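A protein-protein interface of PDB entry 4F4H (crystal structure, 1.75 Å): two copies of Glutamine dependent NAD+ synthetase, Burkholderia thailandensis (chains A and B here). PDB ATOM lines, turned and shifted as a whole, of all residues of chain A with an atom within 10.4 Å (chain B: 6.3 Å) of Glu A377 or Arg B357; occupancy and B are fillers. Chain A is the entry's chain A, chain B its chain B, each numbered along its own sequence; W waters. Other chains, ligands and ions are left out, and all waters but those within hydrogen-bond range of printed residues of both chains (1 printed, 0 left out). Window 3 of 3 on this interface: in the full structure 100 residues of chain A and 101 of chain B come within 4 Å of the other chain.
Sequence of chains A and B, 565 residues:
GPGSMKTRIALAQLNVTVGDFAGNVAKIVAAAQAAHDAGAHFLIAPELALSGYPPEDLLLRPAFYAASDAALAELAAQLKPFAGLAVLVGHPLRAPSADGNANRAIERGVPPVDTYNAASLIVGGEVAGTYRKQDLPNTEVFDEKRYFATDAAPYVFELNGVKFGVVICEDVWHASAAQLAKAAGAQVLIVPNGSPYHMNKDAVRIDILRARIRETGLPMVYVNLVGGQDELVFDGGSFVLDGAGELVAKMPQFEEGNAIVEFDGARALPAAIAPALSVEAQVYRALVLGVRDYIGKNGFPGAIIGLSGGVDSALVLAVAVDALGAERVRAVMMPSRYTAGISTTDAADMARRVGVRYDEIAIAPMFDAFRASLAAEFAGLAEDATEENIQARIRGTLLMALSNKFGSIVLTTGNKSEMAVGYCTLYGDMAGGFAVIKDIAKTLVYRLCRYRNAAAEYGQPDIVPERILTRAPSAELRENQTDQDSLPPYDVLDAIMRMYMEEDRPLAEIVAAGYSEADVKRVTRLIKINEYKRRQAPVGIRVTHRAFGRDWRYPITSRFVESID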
ATOM      1  N   PHE A 370      19.714 -22.778 -28.601  1.00  0.00           N
ATOM      2  CA  PHE A 370      21.123 -23.028 -28.226  1.00  0.00           C
ATOM      3  C   PHE A 370      21.285 -23.217 -26.713  1.00  0.00           C
ATOM      4  O   PHE A 370      21.953 -24.155 -26.261  1.00  0.00           O
ATOM      5  CB  PHE A 370      22.041 -21.900 -28.678  1.00  0.00           C
ATOM      6  CG  PHE A 370      22.479 -21.996 -30.122  1.00  0.00           C
ATOM      7  CD1 PHE A 370      23.460 -22.921 -30.511  1.00  0.00           C
ATOM      8  CD2 PHE A 370      21.963 -21.157 -31.065  1.00  0.00           C
ATOM      9  CE1 PHE A 370      23.880 -23.002 -31.819  1.00  0.00           C
ATOM     10  CE2 PHE A 370      22.382 -21.226 -32.379  1.00  0.00           C
ATOM     11  CZ  PHE A 370      23.337 -22.160 -32.761  1.00  0.00           C
ATOM     12  N   ARG A 371      20.672 -22.325 -25.932  1.00  0.00           N
ATOM     13  CA  ARG A 371      20.777 -22.412 -24.468  1.00  0.00           C
ATOM     14  C   ARG A 371      20.260 -23.758 -23.939  1.00  0.00           C
ATOM     15  O   ARG A 371      20.881 -24.359 -23.056  1.00  0.00           O
ATOM     16  CB  ARG A 371      20.049 -21.248 -23.783  1.00  0.00           C
ATOM     17  N   ALA A 372      19.127 -24.220 -24.465  1.00  0.00           N
ATOM     18  CA  ALA A 372      18.541 -25.501 -24.020  1.00  0.00           C
ATOM     19  C   ALA A 372      19.442 -26.665 -24.415  1.00  0.00           C
ATOM     20  O   ALA A 372      19.606 -27.629 -23.634  1.00  0.00           O
ATOM     21  CB  ALA A 372      17.140 -25.692 -24.599  1.00  0.00           C
ATOM     22  N   SER A 373      20.047 -26.582 -25.605  1.00  0.00           N
ATOM     23  CA  SER A 373      20.924 -27.633 -26.082  1.00  0.00           C
ATOM     24  C   SER A 373      22.205 -27.748 -25.242  1.00  0.00           C
ATOM     25  O   SER A 373      22.767 -28.830 -25.132  1.00  0.00           O
ATOM     26  CB  SER A 373      21.266 -27.466 -27.573  1.00  0.00           C
ATOM     27  OG  SER A 373      22.261 -26.444 -27.780  1.00  0.00           O
ATOM     28  N   LEU A 374      22.645 -26.639 -24.644  1.00  0.00           N
ATOM     29  CA  LEU A 374      23.849 -26.587 -23.832  1.00  0.00           C
ATOM     30  C   LEU A 374      23.567 -26.600 -22.327  1.00  0.00           C
ATOM     31  O   LEU A 374      24.491 -26.551 -21.533  1.00  0.00           O
ATOM     32  CB  LEU A 374      24.649 -25.332 -24.185  1.00  0.00           C
ATOM     33  CG  LEU A 374      25.291 -25.355 -25.577  1.00  0.00           C
ATOM     34  CD1 LEU A 374      25.563 -23.927 -26.057  1.00  0.00           C
ATOM     35  CD2 LEU A 374      26.575 -26.193 -25.568  1.00  0.00           C
ATOM     36  N   ALA A 375      22.298 -26.698 -21.927  1.00  0.00           N
ATOM     37  CA  ALA A 375      21.951 -26.547 -20.519  1.00  0.00           C
ATOM     38  C   ALA A 375      22.632 -27.589 -19.615  1.00  0.00           C
ATOM     39  O   ALA A 375      23.057 -27.267 -18.520  1.00  0.00           O
ATOM     40  CB  ALA A 375      20.417 -26.587 -20.329  1.00  0.00           C
ATOM     41  N   ALA A 376      22.730 -28.830 -20.068  1.00  0.00           N
ATOM     42  CA  ALA A 376      23.376 -29.871 -19.269  1.00  0.00           C
ATOM     43  C   ALA A 376      24.879 -29.589 -19.124  1.00  0.00           C
ATOM     44  O   ALA A 376      25.447 -29.668 -18.026  1.00  0.00           O
ATOM     45  CB  ALA A 376      23.152 -31.239 -19.896  1.00  0.00           C
ATOM     46  N   GLU A 377      25.504 -29.233 -20.240  1.00  0.00           N
ATOM     47  CA  GLU A 377      26.910 -28.906 -20.259  1.00  0.00           C
ATOM     48  C   GLU A 377      27.216 -27.705 -19.350  1.00  0.00           C
ATOM     49  O   GLU A 377      28.231 -27.698 -18.641  1.00  0.00           O
ATOM     50  CB  GLU A 377      27.325 -28.606 -21.709  1.00  0.00           C
ATOM     51  CG  GLU A 377      28.789 -28.341 -21.915  1.00  0.00           C
ATOM     52  CD  GLU A 377      29.580 -29.614 -22.116  1.00  0.00           C
ATOM     53  OE1 GLU A 377      29.008 -30.594 -22.630  1.00  0.00           O
ATOM     54  OE2 GLU A 377      30.764 -29.621 -21.751  1.00  0.00           O
ATOM     55  N   PHE A 378      26.347 -26.690 -19.358  1.00  0.00           N
ATOM     56  CA  PHE A 378      26.641 -25.446 -18.635  1.00  0.00           C
ATOM     57  C   PHE A 378      25.929 -25.364 -17.275  1.00  0.00           C
ATOM     58  O   PHE A 378      25.890 -24.281 -16.662  1.00  0.00           O
ATOM     59  CB  PHE A 378      26.251 -24.226 -19.474  1.00  0.00           C
ATOM     60  CG  PHE A 378      27.080 -24.034 -20.755  1.00  0.00           C
ATOM     61  CD1 PHE A 378      28.219 -24.788 -21.022  1.00  0.00           C
ATOM     62  CD2 PHE A 378      26.709 -23.063 -21.669  1.00  0.00           C
ATOM     63  CE1 PHE A 378      28.957 -24.570 -22.201  1.00  0.00           C
ATOM     64  CE2 PHE A 378      27.438 -22.833 -22.831  1.00  0.00           C
ATOM     65  CZ  PHE A 378      28.565 -23.598 -23.094  1.00  0.00           C
ATOM     66  N   ALA A 379      25.386 -26.488 -16.830  1.00  0.00           N
ATOM     67  CA  ALA A 379      24.626 -26.565 -15.564  1.00  0.00           C
ATOM     68  C   ALA A 379      25.436 -25.979 -14.412  1.00  0.00           C
ATOM     69  O   ALA A 379      26.578 -26.369 -14.202  1.00  0.00           O
ATOM     70  CB  ALA A 379      24.247 -28.007 -15.273  1.00  0.00           C
ATOM     71  N   GLY A 380      24.854 -25.005 -13.710  1.00  0.00           N
ATOM     72  CA  GLY A 380      25.492 -24.387 -12.546  1.00  0.00           C
ATOM     73  C   GLY A 380      26.383 -23.192 -12.828  1.00  0.00           C
ATOM     74  O   GLY A 380      26.835 -22.532 -11.894  1.00  0.00           O
ATOM     75  N   LEU A 381      26.650 -22.904 -14.103  1.00  0.00           N
ATOM     76  CA  LEU A 381      27.530 -21.796 -14.473  1.00  0.00           C
ATOM     77  C   LEU A 381      26.749 -20.535 -14.833  1.00  0.00           C
ATOM     78  O   LEU A 381      25.672 -20.604 -15.418  1.00  0.00           O
ATOM     79  CB  LEU A 381      28.427 -22.212 -15.666  1.00  0.00           C
ATOM     80  CG  LEU A 381      29.161 -23.557 -15.520  1.00  0.00           C
ATOM     81  CD1 LEU A 381      29.908 -23.935 -16.798  1.00  0.00           C
ATOM     82  CD2 LEU A 381      30.121 -23.481 -14.346  1.00  0.00           C
ATOM     83  N   ALA A 382      27.301 -19.381 -14.481  1.00  0.00           N
ATOM     84  CA  ALA A 382      26.741 -18.096 -14.872  1.00  0.00           C
ATOM     85  C   ALA A 382      26.794 -17.942 -16.390  1.00  0.00           C
ATOM     86  O   ALA A 382      27.697 -18.488 -17.051  1.00  0.00           O
ATOM     87  CB  ALA A 382      27.515 -16.962 -14.220  1.00  0.00           C
ATOM     88  N   THR A 386      30.483 -16.223 -23.202  1.00  0.00           N
ATOM     89  CA  THR A 386      30.170 -17.379 -24.059  1.00  0.00           C
ATOM     90  C   THR A 386      28.773 -17.192 -24.684  1.00  0.00           C
ATOM     91  O   THR A 386      28.594 -17.354 -25.889  1.00  0.00           O
ATOM     92  CB  THR A 386      30.233 -18.686 -23.266  1.00  0.00           C
ATOM     93  OG1 THR A 386      31.585 -18.932 -22.846  1.00  0.00           O
ATOM     94  CG2 THR A 386      29.732 -19.906 -24.104  1.00  0.00           C
ATOM     95  N   GLU A 387      27.798 -16.801 -23.869  1.00  0.00           N
ATOM     96  CA  GLU A 387      26.437 -16.652 -24.372  1.00  0.00           C
ATOM     97  C   GLU A 387      26.270 -15.383 -25.224  1.00  0.00           C
ATOM     98  O   GLU A 387      25.492 -15.378 -26.207  1.00  0.00           O
ATOM     99  CB  GLU A 387      25.423 -16.726 -23.222  1.00  0.00           C
ATOM    100  CG  GLU A 387      25.283 -18.129 -22.645  1.00  0.00           C
ATOM    101  CD  GLU A 387      26.353 -18.484 -21.584  1.00  0.00           C
ATOM    102  OE1 GLU A 387      27.235 -17.665 -21.292  1.00  0.00           O
ATOM    103  OE2 GLU A 387      26.283 -19.589 -21.009  1.00  0.00           O
ATOM    104  N   ILE A 390      27.431 -16.465 -28.612  1.00  0.00           N
ATOM    105  CA  ILE A 390      26.441 -17.284 -29.292  1.00  0.00           C
ATOM    106  C   ILE A 390      25.482 -16.340 -30.011  1.00  0.00           C
ATOM    107  O   ILE A 390      25.139 -16.547 -31.170  1.00  0.00           O
ATOM    108  CB  ILE A 390      25.668 -18.223 -28.313  1.00  0.00           C
ATOM    109  CG1 ILE A 390      26.598 -19.311 -27.748  1.00  0.00           C
ATOM    110  CG2 ILE A 390      24.466 -18.851 -29.006  1.00  0.00           C
ATOM    111  CD1 ILE A 390      25.968 -20.100 -26.597  1.00  0.00           C
ATOM    112  N   ALA B 326      44.212 -39.126 -24.767  1.00  0.00           N
ATOM    113  CA  ALA B 326      42.755 -39.118 -24.791  1.00  0.00           C
ATOM    114  C   ALA B 326      42.129 -38.227 -23.754  1.00  0.00           C
ATOM    115  O   ALA B 326      41.086 -37.675 -23.998  1.00  0.00           O
ATOM    116  CB  ALA B 326      42.205 -40.556 -24.621  1.00  0.00           C
ATOM    117  N   VAL B 329      41.259 -34.745 -25.026  1.00  0.00           N
ATOM    118  CA  VAL B 329      40.457 -34.642 -26.254  1.00  0.00           C
ATOM    119  C   VAL B 329      38.991 -34.988 -25.975  1.00  0.00           C
ATOM    120  O   VAL B 329      38.705 -35.943 -25.290  1.00  0.00           O
ATOM    121  CB  VAL B 329      41.004 -35.603 -27.331  1.00  0.00           C
ATOM    122  CG1 VAL B 329      40.190 -35.509 -28.619  1.00  0.00           C
ATOM    123  CG2 VAL B 329      42.471 -35.296 -27.580  1.00  0.00           C
ATOM    124  N   ARG B 330      38.065 -34.219 -26.527  1.00  0.00           N
ATOM    125  CA  ARG B 330      36.660 -34.644 -26.527  1.00  0.00           C
ATOM    126  C   ARG B 330      36.084 -34.619 -27.926  1.00  0.00           C
ATOM    127  O   ARG B 330      36.525 -33.844 -28.761  1.00  0.00           O
ATOM    128  CB  ARG B 330      35.824 -33.812 -25.562  1.00  0.00           C
ATOM    129  CG  ARG B 330      35.640 -32.367 -25.941  1.00  0.00           C
ATOM    130  CD  ARG B 330      34.894 -31.598 -24.862  1.00  0.00           C
ATOM    131  NE  ARG B 330      33.498 -32.031 -24.776  1.00  0.00           N
ATOM    132  CZ  ARG B 330      32.551 -31.432 -24.050  1.00  0.00           C
ATOM    133  NH1 ARG B 330      32.823 -30.348 -23.331  1.00  0.00           N
ATOM    134  NH2 ARG B 330      31.321 -31.918 -24.060  1.00  0.00           N
ATOM    135  N   ALA B 331      35.068 -35.459 -28.156  1.00  0.00           N
ATOM    136  CA  ALA B 331      34.436 -35.577 -29.463  1.00  0.00           C
ATOM    137  C   ALA B 331      32.965 -35.209 -29.329  1.00  0.00           C
ATOM    138  O   ALA B 331      32.304 -35.598 -28.363  1.00  0.00           O
ATOM    139  CB  ALA B 331      34.570 -37.001 -30.008  1.00  0.00           C
ATOM    140  N   VAL B 332      32.448 -34.492 -30.307  1.00  0.00           N
ATOM    141  CA  VAL B 332      31.031 -34.071 -30.284  1.00  0.00           C
ATOM    142  C   VAL B 332      30.397 -34.366 -31.638  1.00  0.00           C
ATOM    143  O   VAL B 332      30.876 -33.909 -32.666  1.00  0.00           O
ATOM    144  CB  VAL B 332      30.890 -32.554 -29.956  1.00  0.00           C
ATOM    145  CG1 VAL B 332      29.411 -32.171 -29.797  1.00  0.00           C
ATOM    146  CG2 VAL B 332      31.706 -32.153 -28.729  1.00  0.00           C
ATOM    147  N   ALA B 351      35.068 -43.003 -31.068  1.00  0.00           N
ATOM    148  CA  ALA B 351      35.358 -42.355 -29.778  1.00  0.00           C
ATOM    149  C   ALA B 351      35.616 -43.380 -28.703  1.00  0.00           C
ATOM    150  O   ALA B 351      36.513 -43.212 -27.903  1.00  0.00           O
ATOM    151  CB  ALA B 351      34.218 -41.409 -29.368  1.00  0.00           C
ATOM    152  N   GLY B 355      39.022 -44.039 -26.517  1.00  0.00           N
ATOM    153  CA  GLY B 355      38.758 -43.715 -25.113  1.00  0.00           C
ATOM    154  C   GLY B 355      38.557 -42.246 -24.810  1.00  0.00           C
ATOM    155  O   GLY B 355      38.939 -41.774 -23.712  1.00  0.00           O
ATOM    156  N   VAL B 356      37.925 -41.509 -25.736  1.00  0.00           N
ATOM    157  CA  VAL B 356      37.639 -40.092 -25.499  1.00  0.00           C
ATOM    158  C   VAL B 356      36.170 -39.867 -25.096  1.00  0.00           C
ATOM    159  O   VAL B 356      35.282 -40.589 -25.509  1.00  0.00           O
ATOM    160  CB  VAL B 356      37.961 -39.206 -26.714  1.00  0.00           C
ATOM    161  CG1 VAL B 356      39.465 -39.264 -27.061  1.00  0.00           C
ATOM    162  CG2 VAL B 356      37.102 -39.579 -27.902  1.00  0.00           C
ATOM    163  N   ARG B 357      35.961 -38.854 -24.273  1.00  0.00           N
ATOM    164  CA  ARG B 357      34.654 -38.339 -23.985  1.00  0.00           C
ATOM    165  C   ARG B 357      33.883 -38.071 -25.283  1.00  0.00           C
ATOM    166  O   ARG B 357      34.441 -37.451 -26.228  1.00  0.00           O
ATOM    167  CB  ARG B 357      34.799 -37.059 -23.208  1.00  0.00           C
ATOM    168  CG  ARG B 357      33.494 -36.377 -22.931  1.00  0.00           C
ATOM    169  CD  ARG B 357      33.702 -35.105 -22.152  1.00  0.00           C
ATOM    170  NE  ARG B 357      32.402 -34.600 -21.708  1.00  0.00           N
ATOM    171  CZ  ARG B 357      32.229 -33.462 -21.054  1.00  0.00           C
ATOM    172  NH1 ARG B 357      33.276 -32.696 -20.764  1.00  0.00           N
ATOM    173  NH2 ARG B 357      31.001 -33.089 -20.705  1.00  0.00           N
ATOM    174  N   TYR B 358      32.627 -38.533 -25.333  1.00  0.00           N
ATOM    175  CA  TYR B 358      31.785 -38.402 -26.518  1.00  0.00           C
ATOM    176  C   TYR B 358      30.417 -37.891 -26.112  1.00  0.00           C
ATOM    177  O   TYR B 358      29.823 -38.459 -25.208  1.00  0.00           O
ATOM    178  CB  TYR B 358      31.628 -39.749 -27.189  1.00  0.00           C
ATOM    179  CG  TYR B 358      30.657 -39.787 -28.347  1.00  0.00           C
ATOM    180  CD1 TYR B 358      31.050 -39.377 -29.628  1.00  0.00           C
ATOM    181  CD2 TYR B 358      29.364 -40.257 -28.190  1.00  0.00           C
ATOM    182  CE1 TYR B 358      30.187 -39.432 -30.706  1.00  0.00           C
ATOM    183  CE2 TYR B 358      28.474 -40.283 -29.261  1.00  0.00           C
ATOM    184  CZ  TYR B 358      28.916 -39.871 -30.525  1.00  0.00           C
ATOM    185  OH  TYR B 358      28.079 -39.923 -31.613  1.00  0.00           O
ATOM    186  N   ASP B 359      29.919 -36.860 -26.800  1.00  0.00           N
ATOM    187  CA  ASP B 359      28.580 -36.307 -26.527  1.00  0.00           C
ATOM    188  C   ASP B 359      27.862 -36.067 -27.827  1.00  0.00           C
ATOM    189  O   ASP B 359      28.507 -35.778 -28.855  1.00  0.00           O
ATOM    190  CB  ASP B 359      28.727 -34.989 -25.781  1.00  0.00           C
ATOM    191  CG  ASP B 359      29.165 -35.181 -24.337  1.00  0.00           C
ATOM    192  OD1 ASP B 359      28.306 -35.590 -23.531  1.00  0.00           O
ATOM    193  OD2 ASP B 359      30.353 -34.942 -23.997  1.00  0.00           O
ATOM    194  N   ILE B 361      24.766 -33.737 -29.540  1.00  0.00           N
ATOM    195  CA  ILE B 361      23.897 -32.565 -29.385  1.00  0.00           C
ATOM    196  C   ILE B 361      23.063 -32.398 -30.644  1.00  0.00           C
ATOM    197  O   ILE B 361      23.601 -32.099 -31.726  1.00  0.00           O
ATOM    198  CB  ILE B 361      24.691 -31.267 -29.143  1.00  0.00           C
ATOM    199  CG1 ILE B 361      25.546 -31.368 -27.885  1.00  0.00           C
ATOM    200  CG2 ILE B 361      23.734 -30.081 -29.019  1.00  0.00           C
ATOM    201  CD1 ILE B 361      26.488 -30.165 -27.684  1.00  0.00           C
ATOM    202  N   LEU B 402      31.487 -24.466 -26.556  1.00  0.00           N
ATOM    203  CA  LEU B 402      32.197 -25.337 -25.647  1.00  0.00           C
ATOM    204  C   LEU B 402      33.640 -24.835 -25.461  1.00  0.00           C
ATOM    205  O   LEU B 402      34.198 -24.876 -24.346  1.00  0.00           O
ATOM    206  CB  LEU B 402      32.188 -26.782 -26.145  1.00  0.00           C
ATOM    207  CG  LEU B 402      30.832 -27.438 -26.366  1.00  0.00           C
ATOM    208  CD1 LEU B 402      31.042 -28.808 -27.020  1.00  0.00           C
ATOM    209  CD2 LEU B 402      30.086 -27.532 -25.032  1.00  0.00           C
ATOM    210  N   PHE B 406      35.003 -23.493 -21.670  1.00  0.00           N
ATOM    211  CA  PHE B 406      35.982 -24.329 -20.976  1.00  0.00           C
ATOM    212  C   PHE B 406      37.418 -24.235 -21.463  1.00  0.00           C
ATOM    213  O   PHE B 406      38.306 -24.768 -20.812  1.00  0.00           O
ATOM    214  CB  PHE B 406      35.527 -25.795 -20.979  1.00  0.00           C
ATOM    215  CG  PHE B 406      34.130 -25.999 -20.427  1.00  0.00           C
ATOM    216  CD1 PHE B 406      33.871 -25.793 -19.104  1.00  0.00           C
ATOM    217  CD2 PHE B 406      33.073 -26.378 -21.260  1.00  0.00           C
ATOM    218  CE1 PHE B 406      32.579 -25.966 -18.580  1.00  0.00           C
ATOM    219  CE2 PHE B 406      31.781 -26.544 -20.745  1.00  0.00           C
ATOM    220  CZ  PHE B 406      31.537 -26.339 -19.408  1.00  0.00           C
HETATM  221  O   HOH W   1      32.450 -29.913 -19.696  1.00  0.00           O
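Of the 16 printed residues of chain A, 5 touch a printed residue of chain B.
Printed residues of chain A that touch a printed residue of chain B: Ser A373, Leu A374, Glu A377, Phe A378 and Leu A381.
Hydrophobic or aromatic side chains of chain B within 4 Å of the printed part of chain A: Ile B361, Leu B402 and Phe B406.
Along chain B the printed residues that touch a printed residue of chain A span positions 330 to 406.
Among the printed residues, Asp or Glu carboxylates within 4 Å of a Lys or Arg side-chain nitrogen of the other chain: Glu A377 with Arg B330 (2.7 Å) and Glu A377 with Arg B357 (3.6 Å).
Glu A377 touches just these residues of chain B: Arg B330 (2.7 Å), Arg B357 (3.6 Å), Leu B402 (3.5 Å) and Phe B406 (3.4 Å).
Of chain A, only Glu A377 (3.6 Å) comes within 4 Å of Arg B357.
Arg B330 touches one residue of chain A.
No residue of chain A comes within 4 Å of Ala B331.
No residue of chain A comes within 4 Å of Val B356.
Printed residues of chain A within 4 Å of Phe B406: Glu A377, Phe A378 and Leu A381.
Of the printed residues of chain B, Leu A374 touches Leu B402 (3.8 Å).
Of the printed residues of chain A, Leu B402 touches Leu A374 and Glu A377.
Ala A372 touches none of the printed residues of chain B.
The nearest residue of chain A that does not touch Arg B357 is Ala A376 (7.1 Å).
The guanidinium group of Arg B330 is in salt-bridge range of the side-chain carboxylate of Glu A377, 2.7 Å away.
NH2 of Arg B357 is in salt-bridge range of OE2 of Glu A377.
Ser A373 touches Ile B361 (CB to CG2, 3.9 Å).
CD2 of Leu B402 touches CD2 of Leu A374 (3.8 Å).
Leu B402 touches Glu A377.
CE2 of Phe B406 touches OE2 of Glu A377, at 3.4 Å.
CE2 of Phe B406 touches CE1 of Phe A378, at 3.7 Å.
CE1 of Phe B406 touches CD1 of Leu A381 (3.8 Å).
Water W1 lies within hydrogen-bond range of OE2 of Glu A377 (2.7 Å) and NH1 of Arg B357 (3.1 Å).
The backbone NH (N) of Ala B331 sits at hydrogen-bond distance from the backbone carbonyl oxygen (O) of Arg B357.
The side-chain hydroxyl (OG) of Ser A373 sits at hydrogen-bond distance from the backbone carbonyl oxygen (O) of Phe A370.
NE of Arg B357 lies within salt-bridge range of OD2 of Asp B359, 3.1 Å away.
The guanidinium group (NH2) of Arg B330 is in salt-bridge range of the side-chain carboxylate (OD2) of Asp B359 (3.2 Å).
No position is printed for both chains.
Of the 8 pairs that touch across the chains among the printed residues, none has its exchanged pair printed and touching as well.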
